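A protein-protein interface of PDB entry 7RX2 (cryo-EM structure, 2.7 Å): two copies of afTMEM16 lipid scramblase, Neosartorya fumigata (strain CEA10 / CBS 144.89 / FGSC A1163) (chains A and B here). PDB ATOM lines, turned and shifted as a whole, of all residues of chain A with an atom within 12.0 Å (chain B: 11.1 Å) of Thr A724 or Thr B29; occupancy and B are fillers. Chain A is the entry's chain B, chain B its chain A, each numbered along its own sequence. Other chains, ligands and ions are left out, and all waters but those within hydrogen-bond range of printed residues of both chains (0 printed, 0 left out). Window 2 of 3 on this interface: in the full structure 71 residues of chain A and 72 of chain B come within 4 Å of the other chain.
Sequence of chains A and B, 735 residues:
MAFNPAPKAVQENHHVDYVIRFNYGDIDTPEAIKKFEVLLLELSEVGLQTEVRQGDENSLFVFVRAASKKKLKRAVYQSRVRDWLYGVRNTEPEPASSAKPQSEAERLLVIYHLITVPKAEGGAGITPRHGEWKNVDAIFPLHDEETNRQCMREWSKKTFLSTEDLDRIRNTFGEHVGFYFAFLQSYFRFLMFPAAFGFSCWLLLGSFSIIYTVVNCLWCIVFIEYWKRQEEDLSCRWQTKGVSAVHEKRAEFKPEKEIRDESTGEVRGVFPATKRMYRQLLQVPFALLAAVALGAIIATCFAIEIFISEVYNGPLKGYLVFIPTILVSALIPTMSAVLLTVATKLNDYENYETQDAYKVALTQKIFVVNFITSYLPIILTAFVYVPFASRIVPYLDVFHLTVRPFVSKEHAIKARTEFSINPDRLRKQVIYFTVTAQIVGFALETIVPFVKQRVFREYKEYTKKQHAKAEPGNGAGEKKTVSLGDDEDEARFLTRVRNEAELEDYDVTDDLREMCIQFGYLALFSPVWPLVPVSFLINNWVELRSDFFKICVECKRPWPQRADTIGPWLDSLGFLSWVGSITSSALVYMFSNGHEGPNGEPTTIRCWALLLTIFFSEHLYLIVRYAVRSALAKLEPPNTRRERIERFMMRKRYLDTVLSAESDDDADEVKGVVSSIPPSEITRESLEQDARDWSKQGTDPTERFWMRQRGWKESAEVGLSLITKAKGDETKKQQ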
ATOM      1  N   SER A 715       1.540  25.741  18.980  1.00  0.00           N
ATOM      2  CA  SER A 715       1.848  26.332  17.682  1.00  0.00           C
ATOM      3  C   SER A 715       2.131  25.256  16.646  1.00  0.00           C
ATOM      4  O   SER A 715       1.704  25.375  15.495  1.00  0.00           O
ATOM      5  CB  SER A 715       3.045  27.277  17.793  1.00  0.00           C
ATOM      6  OG  SER A 715       2.876  28.232  18.826  1.00  0.00           O
ATOM      7  N   ALA A 716       2.821  24.192  17.047  1.00  0.00           N
ATOM      8  CA  ALA A 716       3.138  23.102  16.135  1.00  0.00           C
ATOM      9  C   ALA A 716       1.887  22.393  15.625  1.00  0.00           C
ATOM     10  O   ALA A 716       1.840  21.995  14.458  1.00  0.00           O
ATOM     11  CB  ALA A 716       4.067  22.107  16.824  1.00  0.00           C
ATOM     12  N   GLU A 717       0.865  22.223  16.462  1.00  0.00           N
ATOM     13  CA  GLU A 717      -0.344  21.547  16.010  1.00  0.00           C
ATOM     14  C   GLU A 717      -1.298  22.486  15.302  1.00  0.00           C
ATOM     15  O   GLU A 717      -2.032  22.047  14.412  1.00  0.00           O
ATOM     16  CB  GLU A 717      -1.051  20.885  17.195  1.00  0.00           C
ATOM     17  N   VAL A 718      -1.309  23.762  15.678  1.00  0.00           N
ATOM     18  CA  VAL A 718      -2.072  24.745  14.928  1.00  0.00           C
ATOM     19  C   VAL A 718      -1.511  24.886  13.526  1.00  0.00           C
ATOM     20  O   VAL A 718      -2.253  25.177  12.584  1.00  0.00           O
ATOM     21  CB  VAL A 718      -2.074  26.088  15.672  1.00  0.00           C
ATOM     22  CG1 VAL A 718      -2.833  27.123  14.883  1.00  0.00           C
ATOM     23  CG2 VAL A 718      -2.672  25.921  17.062  1.00  0.00           C
ATOM     24  N   GLY A 719      -0.205  24.681  13.359  1.00  0.00           N
ATOM     25  CA  GLY A 719       0.373  24.682  12.030  1.00  0.00           C
ATOM     26  C   GLY A 719       0.044  23.436  11.240  1.00  0.00           C
ATOM     27  O   GLY A 719      -0.101  23.496  10.019  1.00  0.00           O
ATOM     28  N   LEU A 720      -0.079  22.291  11.916  1.00  0.00           N
ATOM     29  CA  LEU A 720      -0.493  21.078  11.218  1.00  0.00           C
ATOM     30  C   LEU A 720      -1.932  21.172  10.737  1.00  0.00           C
ATOM     31  O   LEU A 720      -2.243  20.736   9.624  1.00  0.00           O
ATOM     32  CB  LEU A 720      -0.312  19.866  12.128  1.00  0.00           C
ATOM     33  CG  LEU A 720      -0.747  18.491  11.618  1.00  0.00           C
ATOM     34  CD1 LEU A 720       0.125  17.413  12.224  1.00  0.00           C
ATOM     35  CD2 LEU A 720      -2.201  18.223  11.959  1.00  0.00           C
ATOM     36  N   SER A 721      -2.824  21.727  11.552  1.00  0.00           N
ATOM     37  CA  SER A 721      -4.214  21.829  11.145  1.00  0.00           C
ATOM     38  C   SER A 721      -4.400  22.742   9.944  1.00  0.00           C
ATOM     39  O   SER A 721      -5.336  22.532   9.170  1.00  0.00           O
ATOM     40  CB  SER A 721      -5.063  22.319  12.319  1.00  0.00           C
ATOM     41  OG  SER A 721      -4.689  23.631  12.702  1.00  0.00           O
ATOM     42  N   LEU A 722      -3.526  23.724   9.756  1.00  0.00           N
ATOM     43  CA  LEU A 722      -3.594  24.619   8.612  1.00  0.00           C
ATOM     44  C   LEU A 722      -2.809  24.114   7.419  1.00  0.00           C
ATOM     45  O   LEU A 722      -3.241  24.315   6.282  1.00  0.00           O
ATOM     46  CB  LEU A 722      -3.071  26.005   8.990  1.00  0.00           C
ATOM     47  CG  LEU A 722      -3.955  26.846   9.896  1.00  0.00           C
ATOM     48  CD1 LEU A 722      -3.201  28.081  10.338  1.00  0.00           C
ATOM     49  CD2 LEU A 722      -5.223  27.227   9.172  1.00  0.00           C
ATOM     50  N   ILE A 723      -1.667  23.468   7.647  1.00  0.00           N
ATOM     51  CA  ILE A 723      -0.875  22.959   6.534  1.00  0.00           C
ATOM     52  C   ILE A 723      -1.637  21.869   5.795  1.00  0.00           C
ATOM     53  O   ILE A 723      -1.713  21.872   4.562  1.00  0.00           O
ATOM     54  CB  ILE A 723       0.491  22.457   7.031  1.00  0.00           C
ATOM     55  CG1 ILE A 723       1.365  23.635   7.458  1.00  0.00           C
ATOM     56  CG2 ILE A 723       1.177  21.659   5.954  1.00  0.00           C
ATOM     57  CD1 ILE A 723       2.622  23.235   8.196  1.00  0.00           C
ATOM     58  N   THR A 724      -2.213  20.918   6.534  1.00  0.00           N
ATOM     59  CA  THR A 724      -2.975  19.855   5.887  1.00  0.00           C
ATOM     60  C   THR A 724      -4.260  20.380   5.269  1.00  0.00           C
ATOM     61  O   THR A 724      -4.614  19.989   4.153  1.00  0.00           O
ATOM     62  CB  THR A 724      -3.303  18.745   6.880  1.00  0.00           C
ATOM     63  OG1 THR A 724      -4.359  19.178   7.747  1.00  0.00           O
ATOM     64  CG2 THR A 724      -2.076  18.387   7.703  1.00  0.00           C
ATOM     65  N   LYS A 725      -4.968  21.260   5.975  1.00  0.00           N
ATOM     66  CA  LYS A 725      -6.228  21.779   5.464  1.00  0.00           C
ATOM     67  C   LYS A 725      -6.040  22.555   4.168  1.00  0.00           C
ATOM     68  O   LYS A 725      -6.939  22.566   3.323  1.00  0.00           O
ATOM     69  CB  LYS A 725      -6.888  22.665   6.519  1.00  0.00           C
ATOM     70  CG  LYS A 725      -8.315  23.049   6.215  1.00  0.00           C
ATOM     71  CD  LYS A 725      -8.424  24.380   5.491  1.00  0.00           C
ATOM     72  CE  LYS A 725      -9.884  24.752   5.294  1.00  0.00           C
ATOM     73  NZ  LYS A 725     -10.063  26.034   4.560  1.00  0.00           N
ATOM     74  N   ALA A 726      -4.886  23.190   3.988  1.00  0.00           N
ATOM     75  CA  ALA A 726      -4.647  24.022   2.818  1.00  0.00           C
ATOM     76  C   ALA A 726      -4.184  23.231   1.605  1.00  0.00           C
ATOM     77  O   ALA A 726      -3.984  23.828   0.543  1.00  0.00           O
ATOM     78  CB  ALA A 726      -3.618  25.103   3.149  1.00  0.00           C
ATOM     79  N   LYS A 727      -4.010  21.922   1.731  1.00  0.00           N
ATOM     80  CA  LYS A 727      -3.601  21.090   0.604  1.00  0.00           C
ATOM     81  C   LYS A 727      -4.730  20.174   0.151  1.00  0.00           C
ATOM     82  O   LYS A 727      -5.897  20.417   0.451  1.00  0.00           O
ATOM     83  CB  LYS A 727      -2.374  20.264   0.972  1.00  0.00           C
ATOM     84  CG  LYS A 727      -1.146  21.101   1.214  1.00  0.00           C
ATOM     85  CD  LYS A 727      -0.016  20.278   1.794  1.00  0.00           C
ATOM     86  CE  LYS A 727       1.269  21.084   1.818  1.00  0.00           C
ATOM     87  NZ  LYS A 727       1.636  21.563   0.457  1.00  0.00           N
ATOM     88  N   PHE B  22       6.462  31.298   6.327  1.00  0.00           N
ATOM     89  CA  PHE B  22       6.811  29.929   5.988  1.00  0.00           C
ATOM     90  C   PHE B  22       6.003  29.492   4.775  1.00  0.00           C
ATOM     91  O   PHE B  22       4.775  29.616   4.766  1.00  0.00           O
ATOM     92  CB  PHE B  22       6.547  29.006   7.175  1.00  0.00           C
ATOM     93  CG  PHE B  22       6.966  27.592   6.947  1.00  0.00           C
ATOM     94  CD1 PHE B  22       8.289  27.233   7.031  1.00  0.00           C
ATOM     95  CD2 PHE B  22       6.034  26.623   6.657  1.00  0.00           C
ATOM     96  CE1 PHE B  22       8.673  25.934   6.825  1.00  0.00           C
ATOM     97  CE2 PHE B  22       6.414  25.330   6.451  1.00  0.00           C
ATOM     98  CZ  PHE B  22       7.735  24.983   6.533  1.00  0.00           C
ATOM     99  N   ASN B  23       6.690  28.997   3.755  1.00  0.00           N
ATOM    100  CA  ASN B  23       6.055  28.562   2.522  1.00  0.00           C
ATOM    101  C   ASN B  23       5.924  27.048   2.500  1.00  0.00           C
ATOM    102  O   ASN B  23       6.818  26.332   2.961  1.00  0.00           O
ATOM    103  CB  ASN B  23       6.857  29.009   1.301  1.00  0.00           C
ATOM    104  CG  ASN B  23       6.786  30.492   1.071  1.00  0.00           C
ATOM    105  OD1 ASN B  23       5.849  31.155   1.503  1.00  0.00           O
ATOM    106  ND2 ASN B  23       7.769  31.023   0.369  1.00  0.00           N
ATOM    107  N   TYR B  24       4.812  26.563   1.952  1.00  0.00           N
ATOM    108  CA  TYR B  24       4.661  25.134   1.725  1.00  0.00           C
ATOM    109  C   TYR B  24       4.091  24.821   0.346  1.00  0.00           C
ATOM    110  O   TYR B  24       3.598  23.708   0.137  1.00  0.00           O
ATOM    111  CB  TYR B  24       3.781  24.491   2.807  1.00  0.00           C
ATOM    112  CG  TYR B  24       2.467  25.182   3.068  1.00  0.00           C
ATOM    113  CD1 TYR B  24       1.409  25.063   2.183  1.00  0.00           C
ATOM    114  CD2 TYR B  24       2.274  25.930   4.210  1.00  0.00           C
ATOM    115  CE1 TYR B  24       0.205  25.685   2.420  1.00  0.00           C
ATOM    116  CE2 TYR B  24       1.071  26.552   4.459  1.00  0.00           C
ATOM    117  CZ  TYR B  24       0.043  26.426   3.559  1.00  0.00           C
ATOM    118  OH  TYR B  24      -1.157  27.049   3.798  1.00  0.00           O
ATOM    119  N   GLY B  25       4.144  25.758  -0.598  1.00  0.00           N
ATOM    120  CA  GLY B  25       3.558  25.508  -1.903  1.00  0.00           C
ATOM    121  C   GLY B  25       4.327  24.481  -2.710  1.00  0.00           C
ATOM    122  O   GLY B  25       3.781  23.860  -3.623  1.00  0.00           O
ATOM    123  N   ASP B  26       5.605  24.297  -2.395  1.00  0.00           N
ATOM    124  CA  ASP B  26       6.459  23.357  -3.104  1.00  0.00           C
ATOM    125  C   ASP B  26       6.929  22.215  -2.216  1.00  0.00           C
ATOM    126  O   ASP B  26       7.989  21.639  -2.472  1.00  0.00           O
ATOM    127  CB  ASP B  26       7.663  24.087  -3.694  1.00  0.00           C
ATOM    128  CG  ASP B  26       7.269  25.086  -4.760  1.00  0.00           C
ATOM    129  OD1 ASP B  26       6.204  24.895  -5.386  1.00  0.00           O
ATOM    130  OD2 ASP B  26       8.029  26.054  -4.983  1.00  0.00           O
ATOM    131  N   ILE B  27       6.168  21.878  -1.180  1.00  0.00           N
ATOM    132  CA  ILE B  27       6.570  20.901  -0.178  1.00  0.00           C
ATOM    133  C   ILE B  27       5.385  19.993   0.107  1.00  0.00           C
ATOM    134  O   ILE B  27       4.242  20.457   0.156  1.00  0.00           O
ATOM    135  CB  ILE B  27       7.054  21.593   1.111  1.00  0.00           C
ATOM    136  CG1 ILE B  27       8.412  22.260   0.890  1.00  0.00           C
ATOM    137  CG2 ILE B  27       7.116  20.617   2.253  1.00  0.00           C
ATOM    138  CD1 ILE B  27       9.429  21.377   0.212  1.00  0.00           C
ATOM    139  N   ASP B  28       5.654  18.706   0.291  1.00  0.00           N
ATOM    140  CA  ASP B  28       4.612  17.794   0.732  1.00  0.00           C
ATOM    141  C   ASP B  28       4.456  17.870   2.248  1.00  0.00           C
ATOM    142  O   ASP B  28       5.384  18.229   2.977  1.00  0.00           O
ATOM    143  CB  ASP B  28       4.926  16.362   0.305  1.00  0.00           C
ATOM    144  N   THR B  29       3.257  17.523   2.713  1.00  0.00           N
ATOM    145  CA  THR B  29       2.896  17.628   4.130  1.00  0.00           C
ATOM    146  C   THR B  29       3.868  16.953   5.091  1.00  0.00           C
ATOM    147  O   THR B  29       4.198  17.568   6.114  1.00  0.00           O
ATOM    148  CB  THR B  29       1.488  17.053   4.330  1.00  0.00           C
ATOM    149  OG1 THR B  29       0.614  17.582   3.327  1.00  0.00           O
ATOM    150  CG2 THR B  29       0.958  17.419   5.705  1.00  0.00           C
ATOM    151  N   PRO B  30       4.342  15.725   4.857  1.00  0.00           N
ATOM    152  CA  PRO B  30       5.301  15.136   5.806  1.00  0.00           C
ATOM    153  C   PRO B  30       6.596  15.915   5.914  1.00  0.00           C
ATOM    154  O   PRO B  30       7.176  15.980   7.004  1.00  0.00           O
ATOM    155  CB  PRO B  30       5.535  13.726   5.251  1.00  0.00           C
ATOM    156  CG  PRO B  30       4.357  13.451   4.393  1.00  0.00           C
ATOM    157  CD  PRO B  30       3.941  14.764   3.818  1.00  0.00           C
ATOM    158  N   GLU B  31       7.070  16.519   4.827  1.00  0.00           N
ATOM    159  CA  GLU B  31       8.296  17.300   4.915  1.00  0.00           C
ATOM    160  C   GLU B  31       8.012  18.728   5.358  1.00  0.00           C
ATOM    161  O   GLU B  31       8.876  19.368   5.963  1.00  0.00           O
ATOM    162  CB  GLU B  31       9.026  17.291   3.571  1.00  0.00           C
ATOM    163  CG  GLU B  31      10.492  17.711   3.644  1.00  0.00           C
ATOM    164  CD  GLU B  31      10.696  19.215   3.566  1.00  0.00           C
ATOM    165  OE1 GLU B  31       9.866  19.901   2.945  1.00  0.00           O
ATOM    166  OE2 GLU B  31      11.692  19.711   4.130  1.00  0.00           O
ATOM    167  N   ALA B  32       6.811  19.236   5.080  1.00  0.00           N
ATOM    168  CA  ALA B  32       6.458  20.583   5.510  1.00  0.00           C
ATOM    169  C   ALA B  32       6.385  20.665   7.026  1.00  0.00           C
ATOM    170  O   ALA B  32       7.075  21.478   7.651  1.00  0.00           O
ATOM    171  CB  ALA B  32       5.135  21.007   4.875  1.00  0.00           C
ATOM    172  N   ILE B  33       5.554  19.823   7.642  1.00  0.00           N
ATOM    173  CA  ILE B  33       5.403  19.870   9.092  1.00  0.00           C
ATOM    174  C   ILE B  33       6.648  19.338   9.781  1.00  0.00           C
ATOM    175  O   ILE B  33       6.886  19.612  10.962  1.00  0.00           O
ATOM    176  CB  ILE B  33       4.138  19.108   9.528  1.00  0.00           C
ATOM    177  CG1 ILE B  33       3.889  19.332  11.018  1.00  0.00           C
ATOM    178  CG2 ILE B  33       4.257  17.632   9.210  1.00  0.00           C
ATOM    179  CD1 ILE B  33       3.596  20.764  11.381  1.00  0.00           C
ATOM    180  N   LYS B  34       7.461  18.560   9.068  1.00  0.00           N
ATOM    181  CA  LYS B  34       8.743  18.154   9.627  1.00  0.00           C
ATOM    182  C   LYS B  34       9.657  19.345   9.860  1.00  0.00           C
ATOM    183  O   LYS B  34      10.385  19.368  10.854  1.00  0.00           O
ATOM    184  CB  LYS B  34       9.430  17.145   8.710  1.00  0.00           C
ATOM    185  N   LYS B  35       9.637  20.332   8.964  1.00  0.00           N
ATOM    186  CA  LYS B  35      10.453  21.531   9.095  1.00  0.00           C
ATOM    187  C   LYS B  35       9.768  22.633   9.879  1.00  0.00           C
ATOM    188  O   LYS B  35      10.450  23.492  10.440  1.00  0.00           O
ATOM    189  CB  LYS B  35      10.845  22.070   7.716  1.00  0.00           C
ATOM    190  CG  LYS B  35      11.783  21.157   6.968  1.00  0.00           C
ATOM    191  CD  LYS B  35      13.129  21.097   7.680  1.00  0.00           C
ATOM    192  CE  LYS B  35      14.032  20.035   7.079  1.00  0.00           C
ATOM    193  NZ  LYS B  35      15.376  20.537   6.686  1.00  0.00           N
ATOM    194  N   PHE B  36       8.436  22.633   9.927  1.00  0.00           N
ATOM    195  CA  PHE B  36       7.744  23.605  10.755  1.00  0.00           C
ATOM    196  C   PHE B  36       7.961  23.330  12.233  1.00  0.00           C
ATOM    197  O   PHE B  36       8.009  24.269  13.034  1.00  0.00           O
ATOM    198  CB  PHE B  36       6.258  23.611  10.421  1.00  0.00           C
ATOM    199  CG  PHE B  36       5.528  24.798  10.950  1.00  0.00           C
ATOM    200  CD1 PHE B  36       5.803  26.064  10.474  1.00  0.00           C
ATOM    201  CD2 PHE B  36       4.567  24.648  11.928  1.00  0.00           C
ATOM    202  CE1 PHE B  36       5.129  27.156  10.965  1.00  0.00           C
ATOM    203  CE2 PHE B  36       3.894  25.729  12.421  1.00  0.00           C
ATOM    204  CZ  PHE B  36       4.175  26.987  11.940  1.00  0.00           C
ATOM    205  N   GLU B  37       8.103  22.060  12.615  1.00  0.00           N
ATOM    206  CA  GLU B  37       8.403  21.746  14.009  1.00  0.00           C
ATOM    207  C   GLU B  37       9.755  22.296  14.417  1.00  0.00           C
ATOM    208  O   GLU B  37       9.882  22.911  15.480  1.00  0.00           O
ATOM    209  CB  GLU B  37       8.369  20.239  14.247  1.00  0.00           C
ATOM    210  CG  GLU B  37       6.993  19.617  14.255  1.00  0.00           C
ATOM    211  CD  GLU B  37       7.040  18.126  14.524  1.00  0.00           C
ATOM    212  OE1 GLU B  37       8.151  17.554  14.536  1.00  0.00           O
ATOM    213  OE2 GLU B  37       5.967  17.526  14.740  1.00  0.00           O
ATOM    214  N   VAL B  38      10.786  22.069  13.600  1.00  0.00           N
ATOM    215  CA  VAL B  38      12.115  22.546  13.960  1.00  0.00           C
ATOM    216  C   VAL B  38      12.161  24.063  13.941  1.00  0.00           C
ATOM    217  O   VAL B  38      12.872  24.679  14.739  1.00  0.00           O
ATOM    218  CB  VAL B  38      13.188  21.934  13.045  1.00  0.00           C
ATOM    219  CG1 VAL B  38      13.297  20.444  13.273  1.00  0.00           C
ATOM    220  CG2 VAL B  38      12.874  22.220  11.605  1.00  0.00           C
ATOM    221  N   VAL B  52       1.197  31.262  15.447  1.00  0.00           N
ATOM    222  CA  VAL B  52       1.091  30.871  14.049  1.00  0.00           C
ATOM    223  C   VAL B  52      -0.287  31.259  13.537  1.00  0.00           C
ATOM    224  O   VAL B  52      -1.287  31.084  14.239  1.00  0.00           O
ATOM    225  CB  VAL B  52       1.337  29.368  13.868  1.00  0.00           C
ATOM    226  CG1 VAL B  52       1.121  28.978  12.431  1.00  0.00           C
ATOM    227  CG2 VAL B  52       2.729  29.015  14.311  1.00  0.00           C
ATOM    228  N   GLN B  54      -2.528  31.956   9.438  1.00  0.00           N
ATOM    229  CA  GLN B  54      -2.493  31.704   8.006  1.00  0.00           C
ATOM    230  C   GLN B  54      -1.935  32.916   7.276  1.00  0.00           C
ATOM    231  O   GLN B  54      -2.428  34.033   7.437  1.00  0.00           O
ATOM    232  CB  GLN B  54      -3.889  31.376   7.486  1.00  0.00           C
ATOM    233  CG  GLN B  54      -3.927  30.996   6.018  1.00  0.00           C
ATOM    234  CD  GLN B  54      -3.532  29.553   5.793  1.00  0.00           C
ATOM    235  OE1 GLN B  54      -3.871  28.682   6.586  1.00  0.00           O
ATOM    236  NE2 GLN B  54      -2.809  29.294   4.716  1.00  0.00           N
ATOM    237  N   ASP B  56      -1.079  32.997   3.505  1.00  0.00           N
ATOM    238  CA  ASP B  56      -1.550  33.138   2.136  1.00  0.00           C
ATOM    239  C   ASP B  56      -2.369  31.900   1.803  1.00  0.00           C
ATOM    240  O   ASP B  56      -2.781  31.140   2.686  1.00  0.00           O
ATOM    241  CB  ASP B  56      -0.375  33.305   1.161  1.00  0.00           C
ATOM    242  CG  ASP B  56       0.403  34.562   1.403  1.00  0.00           C
ATOM    243  OD1 ASP B  56      -0.216  35.588   1.752  1.00  0.00           O
ATOM    244  OD2 ASP B  56       1.639  34.526   1.244  1.00  0.00           O
ATOM    245  N   GLU B  57      -2.623  31.698   0.514  1.00  0.00           N
ATOM    246  CA  GLU B  57      -3.154  30.416   0.081  1.00  0.00           C
ATOM    247  C   GLU B  57      -2.095  29.329   0.169  1.00  0.00           C
ATOM    248  O   GLU B  57      -2.429  28.140   0.161  1.00  0.00           O
ATOM    249  CB  GLU B  57      -3.694  30.527  -1.341  1.00  0.00           C
ATOM    250  N   ASN B  58      -0.816  29.710   0.249  1.00  0.00           N
ATOM    251  CA  ASN B  58       0.274  28.746   0.288  1.00  0.00           C
ATOM    252  C   ASN B  58       1.358  29.104   1.299  1.00  0.00           C
ATOM    253  O   ASN B  58       2.451  28.534   1.236  1.00  0.00           O
ATOM    254  CB  ASN B  58       0.910  28.599  -1.098  1.00  0.00           C
ATOM    255  CG  ASN B  58      -0.108  28.343  -2.187  1.00  0.00           C
ATOM    256  OD1 ASN B  58      -0.611  29.274  -2.809  1.00  0.00           O
ATOM    257  ND2 ASN B  58      -0.417  27.073  -2.424  1.00  0.00           N
ATOM    258  N   SER B  59       1.101  30.026   2.220  1.00  0.00           N
ATOM    259  CA  SER B  59       2.108  30.423   3.190  1.00  0.00           C
ATOM    260  C   SER B  59       1.478  30.562   4.567  1.00  0.00           C
ATOM    261  O   SER B  59       0.302  30.900   4.714  1.00  0.00           O
ATOM    262  CB  SER B  59       2.801  31.729   2.784  1.00  0.00           C
ATOM    263  OG  SER B  59       2.100  32.857   3.261  1.00  0.00           O
ATOM    264  N   LEU B  60       2.294  30.312   5.582  1.00  0.00           N
ATOM    265  CA  LEU B  60       1.823  30.195   6.954  1.00  0.00           C
ATOM    266  C   LEU B  60       2.821  30.926   7.838  1.00  0.00           C
ATOM    267  O   LEU B  60       3.777  30.305   8.305  1.00  0.00           O
ATOM    268  CB  LEU B  60       1.731  28.726   7.336  1.00  0.00           C
ATOM    269  CG  LEU B  60       1.367  28.325   8.755  1.00  0.00           C
ATOM    270  CD1 LEU B  60      -0.123  28.380   8.927  1.00  0.00           C
ATOM    271  CD2 LEU B  60       1.893  26.944   9.035  1.00  0.00           C
ATOM    272  N   ASN B 135      12.272  27.117   2.612  1.00  0.00           N
ATOM    273  CA  ASN B 135      10.852  27.446   2.644  1.00  0.00           C
ATOM    274  C   ASN B 135      10.601  28.764   3.357  1.00  0.00           C
ATOM    275  O   ASN B 135       9.661  29.489   3.018  1.00  0.00           O
ATOM    276  CB  ASN B 135      10.067  26.323   3.309  1.00  0.00           C
ATOM    277  CG  ASN B 135      10.217  25.009   2.587  1.00  0.00           C
ATOM    278  OD1 ASN B 135      10.342  23.957   3.210  1.00  0.00           O
ATOM    279  ND2 ASN B 135      10.200  25.061   1.263  1.00  0.00           N
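Thr A724 touches one residue of chain B.
Thr B29 touches just these residues of chain A: Thr A724 (3.8 Å) and Lys A727 (3.2 Å).
No residue of chain B comes within 4 Å of Ser A721.
Ile A723 touches just one residue of chain B: Leu B60.
Printed residues of chain B within 4 Å of Ala A726: Tyr B24 (3.2 Å).
Lys A727 touches just these residues of chain B: Tyr B24, Ile B27 and Thr B29.
Of chain A, only Lys A727 (2.8 Å) comes within 4 Å of Ile B27.
No residue of chain A comes within 4 Å of Asp B28.
Pro B30 touches none of the printed residues of chain A.
Of the printed residues of chain B, Leu A722 touches Gln B54 (3.3 Å) and Leu B60 (3.4 Å).
Of the printed residues of chain A, Val B52 touches Ser A715.
Printed residues of chain A within 4 Å of Tyr B24: Ala A726 (3.2 Å) and Lys A727 (2.9 Å).
Printed residues of chain B within 4 Å of Gly A719: Phe B36 (3.7 Å).
Of the printed residues of chain B, Ala A716 touches Ile B33.
The nearest residue of chain B that does not touch Thr A724 is Ile B33 (6.5 Å).
The nearest residue of chain A that does not touch Thr B29 is Ile A723 (4.3 Å).
The nearest printed residue of chain A that does not touch Gln B54 is Ala A726 (4.5 Å).
Hydrophobic or aromatic side chains of chain A within 4 Å of the printed part of chain B: Leu A722, Ile A723 and Ala A726.
Along chain A the printed residues that touch a printed residue of chain B span positions 715 to 727.
Of the 25 printed residues of chain B, 8 touch a printed residue of chain A.
Hydrophobic or aromatic side chains of chain B that line the printed part of chain A: Tyr B24, Ile B33, Phe B36, Val B52 and Leu B60.
Among the printed residues, 12 pairs touch across the chains.
Among the printed residues, no Asp or Glu carboxylate lies within 4 Å of a Lys or Arg side-chain nitrogen of the other chain.
The backbone carbonyl oxygen (O) of Phe B22 sits at hydrogen-bond distance from the backbone NH (N) of Leu B60 (2.7 Å).
The backbone carbonyl oxygen (O) of Asn B58 sits at hydrogen-bond distance from the backbone NH (N) of Tyr B24, 3.2 Å away.
NE2 of Gln B54 is in hydrogen-bond range of OH of Tyr B24 (2.9 Å).
The side-chain amide nitrogen of Gln B54 sits at hydrogen-bond distance from the backbone carbonyl oxygen of Asp B56 (2.7 Å).
O of Leu A720 lies close to OG1 of Thr A724 (3.2 Å).
The side-chain amino group (NZ) of Lys A727 sits at hydrogen-bond distance from the backbone carbonyl oxygen (O) of Ile B27 (2.8 Å).
O of Tyr B24 sits at hydrogen-bond distance from NZ of Lys A727, at 2.9 Å.
No position is printed for both chains.
Of the 12 pairs that touch across the chains among the printed residues, none has its exchanged pair printed and touching as well.
Ser A715 touches Phe B36 (O to CE2, 3.8 Å).
CG2 of Val B52 touches CB of Ser A715, at 3.9 Å.
Ala A716 touches Ile B33.
Gly A719 touches Phe B36 (CA to CE2, 3.7 Å).
CD2 of Leu A722 touches OE1 of Gln B54, 3.3 Å away.
Leu B60 touches Leu A722 (CD1 to CD1, 3.4 Å).
Ile A723 touches Leu B60 (CG1 to CD2, 3.7 Å).
CG2 of Thr A724 touches CG2 of Thr B29 (3.8 Å).
CB of Ala A726 touches OH of Tyr B24 (3.2 Å).
CD of Lys A727 touches OG1 of Thr B29, 3.2 Å away.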
